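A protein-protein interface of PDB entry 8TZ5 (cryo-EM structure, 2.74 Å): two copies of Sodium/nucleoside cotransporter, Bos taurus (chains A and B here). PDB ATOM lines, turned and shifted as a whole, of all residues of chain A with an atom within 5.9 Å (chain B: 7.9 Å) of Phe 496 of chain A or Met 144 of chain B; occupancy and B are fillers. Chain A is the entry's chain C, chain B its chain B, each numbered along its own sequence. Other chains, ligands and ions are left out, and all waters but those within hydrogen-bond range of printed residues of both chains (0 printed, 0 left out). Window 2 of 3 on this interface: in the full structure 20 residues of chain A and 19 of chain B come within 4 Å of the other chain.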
ATOM      1  N   LEU A 492     -19.446  21.619  -8.215  1.00  0.00           N
ATOM      2  CA  LEU A 492     -18.771  21.089  -9.396  1.00  0.00           C
ATOM      3  C   LEU A 492     -19.760  20.414 -10.339  1.00  0.00           C
ATOM      4  O   LEU A 492     -19.690  20.590 -11.560  1.00  0.00           O
ATOM      5  CB  LEU A 492     -17.674  20.111  -8.977  1.00  0.00           C
ATOM      6  CG  LEU A 492     -17.000  19.325 -10.105  1.00  0.00           C
ATOM      7  CD1 LEU A 492     -16.305  20.263 -11.078  1.00  0.00           C
ATOM      8  CD2 LEU A 492     -16.018  18.313  -9.539  1.00  0.00           C
ATOM      9  N   GLY A 493     -20.689  19.632  -9.787  1.00  0.00           N
ATOM     10  CA  GLY A 493     -21.618  18.896 -10.629  1.00  0.00           C
ATOM     11  C   GLY A 493     -22.486  19.800 -11.482  1.00  0.00           C
ATOM     12  O   GLY A 493     -22.800  19.473 -12.629  1.00  0.00           O
ATOM     13  N   ASN A 494     -22.891  20.949 -10.935  1.00  0.00           N
ATOM     14  CA  ASN A 494     -23.776  21.845 -11.670  1.00  0.00           C
ATOM     15  C   ASN A 494     -23.161  22.321 -12.977  1.00  0.00           C
ATOM     16  O   ASN A 494     -23.897  22.717 -13.887  1.00  0.00           O
ATOM     17  CB  ASN A 494     -24.142  23.052 -10.804  1.00  0.00           C
ATOM     18  CG  ASN A 494     -25.162  23.954 -11.469  1.00  0.00           C
ATOM     19  OD1 ASN A 494     -25.984  23.500 -12.263  1.00  0.00           O
ATOM     20  ND2 ASN A 494     -25.108  25.240 -11.150  1.00  0.00           N
ATOM     21  N   MET A 495     -21.832  22.290 -13.096  1.00  0.00           N
ATOM     22  CA  MET A 495     -21.179  22.689 -14.336  1.00  0.00           C
ATOM     23  C   MET A 495     -21.402  21.690 -15.461  1.00  0.00           C
ATOM     24  O   MET A 495     -21.068  21.995 -16.611  1.00  0.00           O
ATOM     25  CB  MET A 495     -19.680  22.872 -14.099  1.00  0.00           C
ATOM     26  CG  MET A 495     -19.352  23.957 -13.091  1.00  0.00           C
ATOM     27  SD  MET A 495     -17.583  24.156 -12.820  1.00  0.00           S
ATOM     28  CE  MET A 495     -17.590  25.465 -11.601  1.00  0.00           C
ATOM     29  N   PHE A 496     -21.954  20.514 -15.161  1.00  0.00           N
ATOM     30  CA  PHE A 496     -22.301  19.519 -16.167  1.00  0.00           C
ATOM     31  C   PHE A 496     -23.789  19.191 -16.135  1.00  0.00           C
ATOM     32  O   PHE A 496     -24.199  18.126 -16.608  1.00  0.00           O
ATOM     33  CB  PHE A 496     -21.472  18.248 -15.971  1.00  0.00           C
ATOM     34  CG  PHE A 496     -20.000  18.505 -15.814  1.00  0.00           C
ATOM     35  CD1 PHE A 496     -19.179  18.610 -16.922  1.00  0.00           C
ATOM     36  CD2 PHE A 496     -19.438  18.643 -14.556  1.00  0.00           C
ATOM     37  CE1 PHE A 496     -17.826  18.847 -16.781  1.00  0.00           C
ATOM     38  CE2 PHE A 496     -18.085  18.880 -14.409  1.00  0.00           C
ATOM     39  CZ  PHE A 496     -17.279  18.982 -15.522  1.00  0.00           C
ATOM     40  N   ASP A 497     -24.603  20.087 -15.578  1.00  0.00           N
ATOM     41  CA  ASP A 497     -26.045  19.882 -15.451  1.00  0.00           C
ATOM     42  C   ASP A 497     -26.363  18.657 -14.599  1.00  0.00           C
ATOM     43  O   ASP A 497     -27.382  17.992 -14.802  1.00  0.00           O
ATOM     44  CB  ASP A 497     -26.711  19.765 -16.825  1.00  0.00           C
ATOM     45  CG  ASP A 497     -26.553  21.021 -17.657  1.00  0.00           C
ATOM     46  OD1 ASP A 497     -26.497  22.122 -17.070  1.00  0.00           O
ATOM     47  OD2 ASP A 497     -26.484  20.908 -18.899  1.00  0.00           O
ATOM     48  N   TYR A 498     -25.494  18.352 -13.638  1.00  0.00           N
ATOM     49  CA  TYR A 498     -25.689  17.243 -12.705  1.00  0.00           C
ATOM     50  C   TYR A 498     -25.394  17.734 -11.294  1.00  0.00           C
ATOM     51  O   TYR A 498     -24.394  17.346 -10.679  1.00  0.00           O
ATOM     52  CB  TYR A 498     -24.802  16.052 -13.073  1.00  0.00           C
ATOM     53  CG  TYR A 498     -25.133  14.790 -12.309  1.00  0.00           C
ATOM     54  CD1 TYR A 498     -26.364  14.169 -12.459  1.00  0.00           C
ATOM     55  CD2 TYR A 498     -24.211  14.214 -11.444  1.00  0.00           C
ATOM     56  CE1 TYR A 498     -26.672  13.016 -11.765  1.00  0.00           C
ATOM     57  CE2 TYR A 498     -24.511  13.060 -10.747  1.00  0.00           C
ATOM     58  CZ  TYR A 498     -25.743  12.466 -10.913  1.00  0.00           C
ATOM     59  OH  TYR A 498     -26.050  11.317 -10.223  1.00  0.00           O
ATOM     60  N   ALA B 136      -8.649  17.883 -18.251  1.00  0.00           N
ATOM     61  CA  ALA B 136      -9.754  17.501 -19.122  1.00  0.00           C
ATOM     62  C   ALA B 136     -11.090  17.906 -18.514  1.00  0.00           C
ATOM     63  O   ALA B 136     -11.966  18.430 -19.213  1.00  0.00           O
ATOM     64  CB  ALA B 136      -9.717  15.996 -19.383  1.00  0.00           C
ATOM     65  N   LEU B 137     -11.263  17.676 -17.211  1.00  0.00           N
ATOM     66  CA  LEU B 137     -12.492  18.103 -16.554  1.00  0.00           C
ATOM     67  C   LEU B 137     -12.674  19.612 -16.662  1.00  0.00           C
ATOM     68  O   LEU B 137     -13.770  20.094 -16.978  1.00  0.00           O
ATOM     69  CB  LEU B 137     -12.480  17.680 -15.084  1.00  0.00           C
ATOM     70  CG  LEU B 137     -12.608  16.188 -14.772  1.00  0.00           C
ATOM     71  CD1 LEU B 137     -12.567  15.964 -13.267  1.00  0.00           C
ATOM     72  CD2 LEU B 137     -13.884  15.614 -15.362  1.00  0.00           C
ATOM     73  N   VAL B 138     -11.604  20.371 -16.419  1.00  0.00           N
ATOM     74  CA  VAL B 138     -11.706  21.828 -16.446  1.00  0.00           C
ATOM     75  C   VAL B 138     -12.075  22.310 -17.844  1.00  0.00           C
ATOM     76  O   VAL B 138     -12.957  23.161 -18.017  1.00  0.00           O
ATOM     77  CB  VAL B 138     -10.393  22.466 -15.957  1.00  0.00           C
ATOM     78  CG1 VAL B 138     -10.421  23.971 -16.176  1.00  0.00           C
ATOM     79  CG2 VAL B 138     -10.164  22.145 -14.490  1.00  0.00           C
ATOM     80  N   ILE B 139     -11.399  21.779 -18.865  1.00  0.00           N
ATOM     81  CA  ILE B 139     -11.648  22.238 -20.229  1.00  0.00           C
ATOM     82  C   ILE B 139     -13.047  21.837 -20.680  1.00  0.00           C
ATOM     83  O   ILE B 139     -13.723  22.595 -21.383  1.00  0.00           O
ATOM     84  CB  ILE B 139     -10.565  21.709 -21.188  1.00  0.00           C
ATOM     85  CG1 ILE B 139     -10.730  22.341 -22.572  1.00  0.00           C
ATOM     86  CG2 ILE B 139     -10.631  20.201 -21.293  1.00  0.00           C
ATOM     87  CD1 ILE B 139      -9.605  22.020 -23.532  1.00  0.00           C
ATOM     88  N   ALA B 140     -13.503  20.641 -20.298  1.00  0.00           N
ATOM     89  CA  ALA B 140     -14.861  20.235 -20.644  1.00  0.00           C
ATOM     90  C   ALA B 140     -15.889  21.147 -19.988  1.00  0.00           C
ATOM     91  O   ALA B 140     -16.868  21.557 -20.627  1.00  0.00           O
ATOM     92  CB  ALA B 140     -15.093  18.781 -20.234  1.00  0.00           C
ATOM     93  N   ALA B 141     -15.682  21.483 -18.712  1.00  0.00           N
ATOM     94  CA  ALA B 141     -16.595  22.398 -18.037  1.00  0.00           C
ATOM     95  C   ALA B 141     -16.610  23.758 -18.724  1.00  0.00           C
ATOM     96  O   ALA B 141     -17.675  24.361 -18.903  1.00  0.00           O
ATOM     97  CB  ALA B 141     -16.203  22.543 -16.568  1.00  0.00           C
ATOM     98  N   CYS B 142     -15.436  24.258 -19.114  1.00  0.00           N
ATOM     99  CA  CYS B 142     -15.380  25.529 -19.829  1.00  0.00           C
ATOM    100  C   CYS B 142     -16.113  25.447 -21.163  1.00  0.00           C
ATOM    101  O   CYS B 142     -16.835  26.377 -21.541  1.00  0.00           O
ATOM    102  CB  CYS B 142     -13.924  25.942 -20.044  1.00  0.00           C
ATOM    103  SG  CYS B 142     -13.079  26.497 -18.545  1.00  0.00           S
ATOM    104  N   VAL B 143     -15.940  24.341 -21.889  1.00  0.00           N
ATOM    105  CA  VAL B 143     -16.583  24.193 -23.193  1.00  0.00           C
ATOM    106  C   VAL B 143     -18.097  24.190 -23.040  1.00  0.00           C
ATOM    107  O   VAL B 143     -18.817  24.861 -23.790  1.00  0.00           O
ATOM    108  CB  VAL B 143     -16.085  22.915 -23.893  1.00  0.00           C
ATOM    109  CG1 VAL B 143     -17.003  22.548 -25.051  1.00  0.00           C
ATOM    110  CG2 VAL B 143     -14.659  23.101 -24.385  1.00  0.00           C
ATOM    111  N   MET B 144     -18.608  23.431 -22.066  1.00  0.00           N
ATOM    112  CA  MET B 144     -20.054  23.365 -21.882  1.00  0.00           C
ATOM    113  C   MET B 144     -20.623  24.731 -21.519  1.00  0.00           C
ATOM    114  O   MET B 144     -21.679  25.127 -22.025  1.00  0.00           O
ATOM    115  CB  MET B 144     -20.402  22.332 -20.810  1.00  0.00           C
ATOM    116  CG  MET B 144     -20.038  20.908 -21.194  1.00  0.00           C
ATOM    117  SD  MET B 144     -20.531  19.696 -19.954  1.00  0.00           S
ATOM    118  CE  MET B 144     -22.314  19.809 -20.065  1.00  0.00           C
ATOM    119  N   ASN B 145     -19.939  25.465 -20.643  1.00  0.00           N
ATOM    120  CA  ASN B 145     -20.362  26.817 -20.284  1.00  0.00           C
ATOM    121  C   ASN B 145     -19.187  27.522 -19.626  1.00  0.00           C
ATOM    122  O   ASN B 145     -18.671  27.044 -18.610  1.00  0.00           O
ATOM    123  CB  ASN B 145     -21.570  26.782 -19.352  1.00  0.00           C
ATOM    124  CG  ASN B 145     -22.186  28.151 -19.140  1.00  0.00           C
ATOM    125  OD1 ASN B 145     -21.513  29.176 -19.259  1.00  0.00           O
ATOM    126  ND2 ASN B 145     -23.475  28.175 -18.822  1.00  0.00           N
ATOM    127  N   PHE B 146     -18.770  28.652 -20.197  1.00  0.00           N
ATOM    128  CA  PHE B 146     -17.573  29.332 -19.711  1.00  0.00           C
ATOM    129  C   PHE B 146     -17.876  30.215 -18.506  1.00  0.00           C
ATOM    130  O   PHE B 146     -17.120  30.220 -17.528  1.00  0.00           O
ATOM    131  CB  PHE B 146     -16.952  30.162 -20.834  1.00  0.00           C
ATOM    132  CG  PHE B 146     -15.578  30.674 -20.516  1.00  0.00           C
ATOM    133  CD1 PHE B 146     -15.408  31.896 -19.886  1.00  0.00           C
ATOM    134  CD2 PHE B 146     -14.457  29.932 -20.841  1.00  0.00           C
ATOM    135  CE1 PHE B 146     -14.144  32.367 -19.589  1.00  0.00           C
ATOM    136  CE2 PHE B 146     -13.191  30.398 -20.548  1.00  0.00           C
ATOM    137  CZ  PHE B 146     -13.034  31.617 -19.922  1.00  0.00           C
ATOM    138  N   HIS B 147     -18.972  30.974 -18.561  1.00  0.00           N
ATOM    139  CA  HIS B 147     -19.296  31.877 -17.461  1.00  0.00           C
ATOM    140  C   HIS B 147     -19.522  31.107 -16.167  1.00  0.00           C
ATOM    141  O   HIS B 147     -19.120  31.556 -15.087  1.00  0.00           O
ATOM    142  CB  HIS B 147     -20.531  32.708 -17.813  1.00  0.00           C
ATOM    143  CG  HIS B 147     -20.933  33.677 -16.745  1.00  0.00           C
ATOM    144  ND1 HIS B 147     -20.113  34.699 -16.318  1.00  0.00           N
ATOM    145  CD2 HIS B 147     -22.071  33.782 -16.019  1.00  0.00           C
ATOM    146  CE1 HIS B 147     -20.727  35.391 -15.376  1.00  0.00           C
ATOM    147  NE2 HIS B 147     -21.917  34.854 -15.174  1.00  0.00           N
ATOM    148  N   ARG B 148     -20.166  29.942 -16.256  1.00  0.00           N
ATOM    149  CA  ARG B 148     -20.448  29.151 -15.064  1.00  0.00           C
ATOM    150  C   ARG B 148     -19.185  28.524 -14.485  1.00  0.00           C
ATOM    151  O   ARG B 148     -19.118  28.279 -13.275  1.00  0.00           O
ATOM    152  CB  ARG B 148     -21.476  28.071 -15.401  1.00  0.00           C
ATOM    153  CG  ARG B 148     -21.924  27.228 -14.221  1.00  0.00           C
ATOM    154  CD  ARG B 148     -23.063  26.300 -14.619  1.00  0.00           C
ATOM    155  NE  ARG B 148     -22.702  25.432 -15.733  1.00  0.00           N
ATOM    156  CZ  ARG B 148     -23.551  24.641 -16.375  1.00  0.00           C
ATOM    157  NH1 ARG B 148     -24.832  24.592 -16.049  1.00  0.00           N
ATOM    158  NH2 ARG B 148     -23.104  23.881 -17.371  1.00  0.00           N
ATOM    159  N   ALA B 149     -18.185  28.256 -15.323  1.00  0.00           N
ATOM    160  CA  ALA B 149     -16.955  27.599 -14.901  1.00  0.00           C
ATOM    161  C   ALA B 149     -15.797  28.571 -14.707  1.00  0.00           C
ATOM    162  O   ALA B 149     -14.651  28.131 -14.571  1.00  0.00           O
ATOM    163  CB  ALA B 149     -16.563  26.525 -15.916  1.00  0.00           C
ATOM    164  N   LEU B 152     -13.314  28.153 -11.507  1.00  0.00           N
ATOM    165  CA  LEU B 152     -12.440  26.991 -11.609  1.00  0.00           C
ATOM    166  C   LEU B 152     -11.276  27.273 -12.549  1.00  0.00           C
ATOM    167  O   LEU B 152     -10.127  26.916 -12.257  1.00  0.00           O
ATOM    168  CB  LEU B 152     -13.239  25.784 -12.095  1.00  0.00           C
ATOM    169  CG  LEU B 152     -12.475  24.467 -12.218  1.00  0.00           C
ATOM    170  CD1 LEU B 152     -11.969  24.006 -10.861  1.00  0.00           C
ATOM    171  CD2 LEU B 152     -13.359  23.409 -12.854  1.00  0.00           C
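Among the printed residues, pairs that only touch across the chains: Met 495 of chain A with Ala 149 of chain B (3.98 Å), Phe 496 of chain A with Leu 137 of chain B (3.96 Å), Phe 496 of chain A with Ala 141 of chain B (3.9 Å) and Phe 496 of chain A with Met 144 of chain B (3.5 Å).
N of Arg 148 of chain B is in hydrogen-bond range of OD1 of Asn 145 of chain B (3.4 Å).
Of the printed residues of chain B, Asn 494 of chain A touches Arg 148. Of the printed residues of chain B, Met 495 of chain A touches Arg 148 and Ala 149. Of chain B, only Leu 137, Ala 141 and Met 144 come within 4 Å of Phe 496 of chain A. Printed residues of chain B within 4 Å of Asp 497 of chain A: Arg 148 (3.1 Å). Of the printed residues of chain A, Leu 137 of chain B touches Phe 496. Met 144 of chain B touches just one residue of chain A: Phe 496 (3.5 Å). Printed residues of chain A within 4 Å of Arg 148 of chain B: Asn 494, Met 495 and Asp 497. The nearest residue of chain A that does not touch Met 144 of chain B is Met 495 of chain A (4.1 Å).
NH1 of Arg 148 of chain B lies within hydrogen-bond range of O of Asn 494 of chain A (3.0 Å). The guanidinium group (NH2) of Arg 148 of chain B lies within hydrogen-bond range of the backbone carbonyl oxygen (O) of Met 495 of chain A, 2.9 Å away. The guanidinium group of Arg 148 of chain B is in salt-bridge range of the side-chain carboxylate of Asp 497 of chain A (3.1 Å).
No position is printed for both chains.
Printed residues of chain B that touch a printed residue of chain A: Leu 137, Ala 141, Met 144, Arg 148 and Ala 149. Among the printed residues, 7 pairs touch across the chains. Among the printed residues, Asp or Glu carboxylates within 4 Å of a Lys or Arg side-chain nitrogen of the other chain: Asp 497 of chain A with Arg 148 of chain B (3.1 Å).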
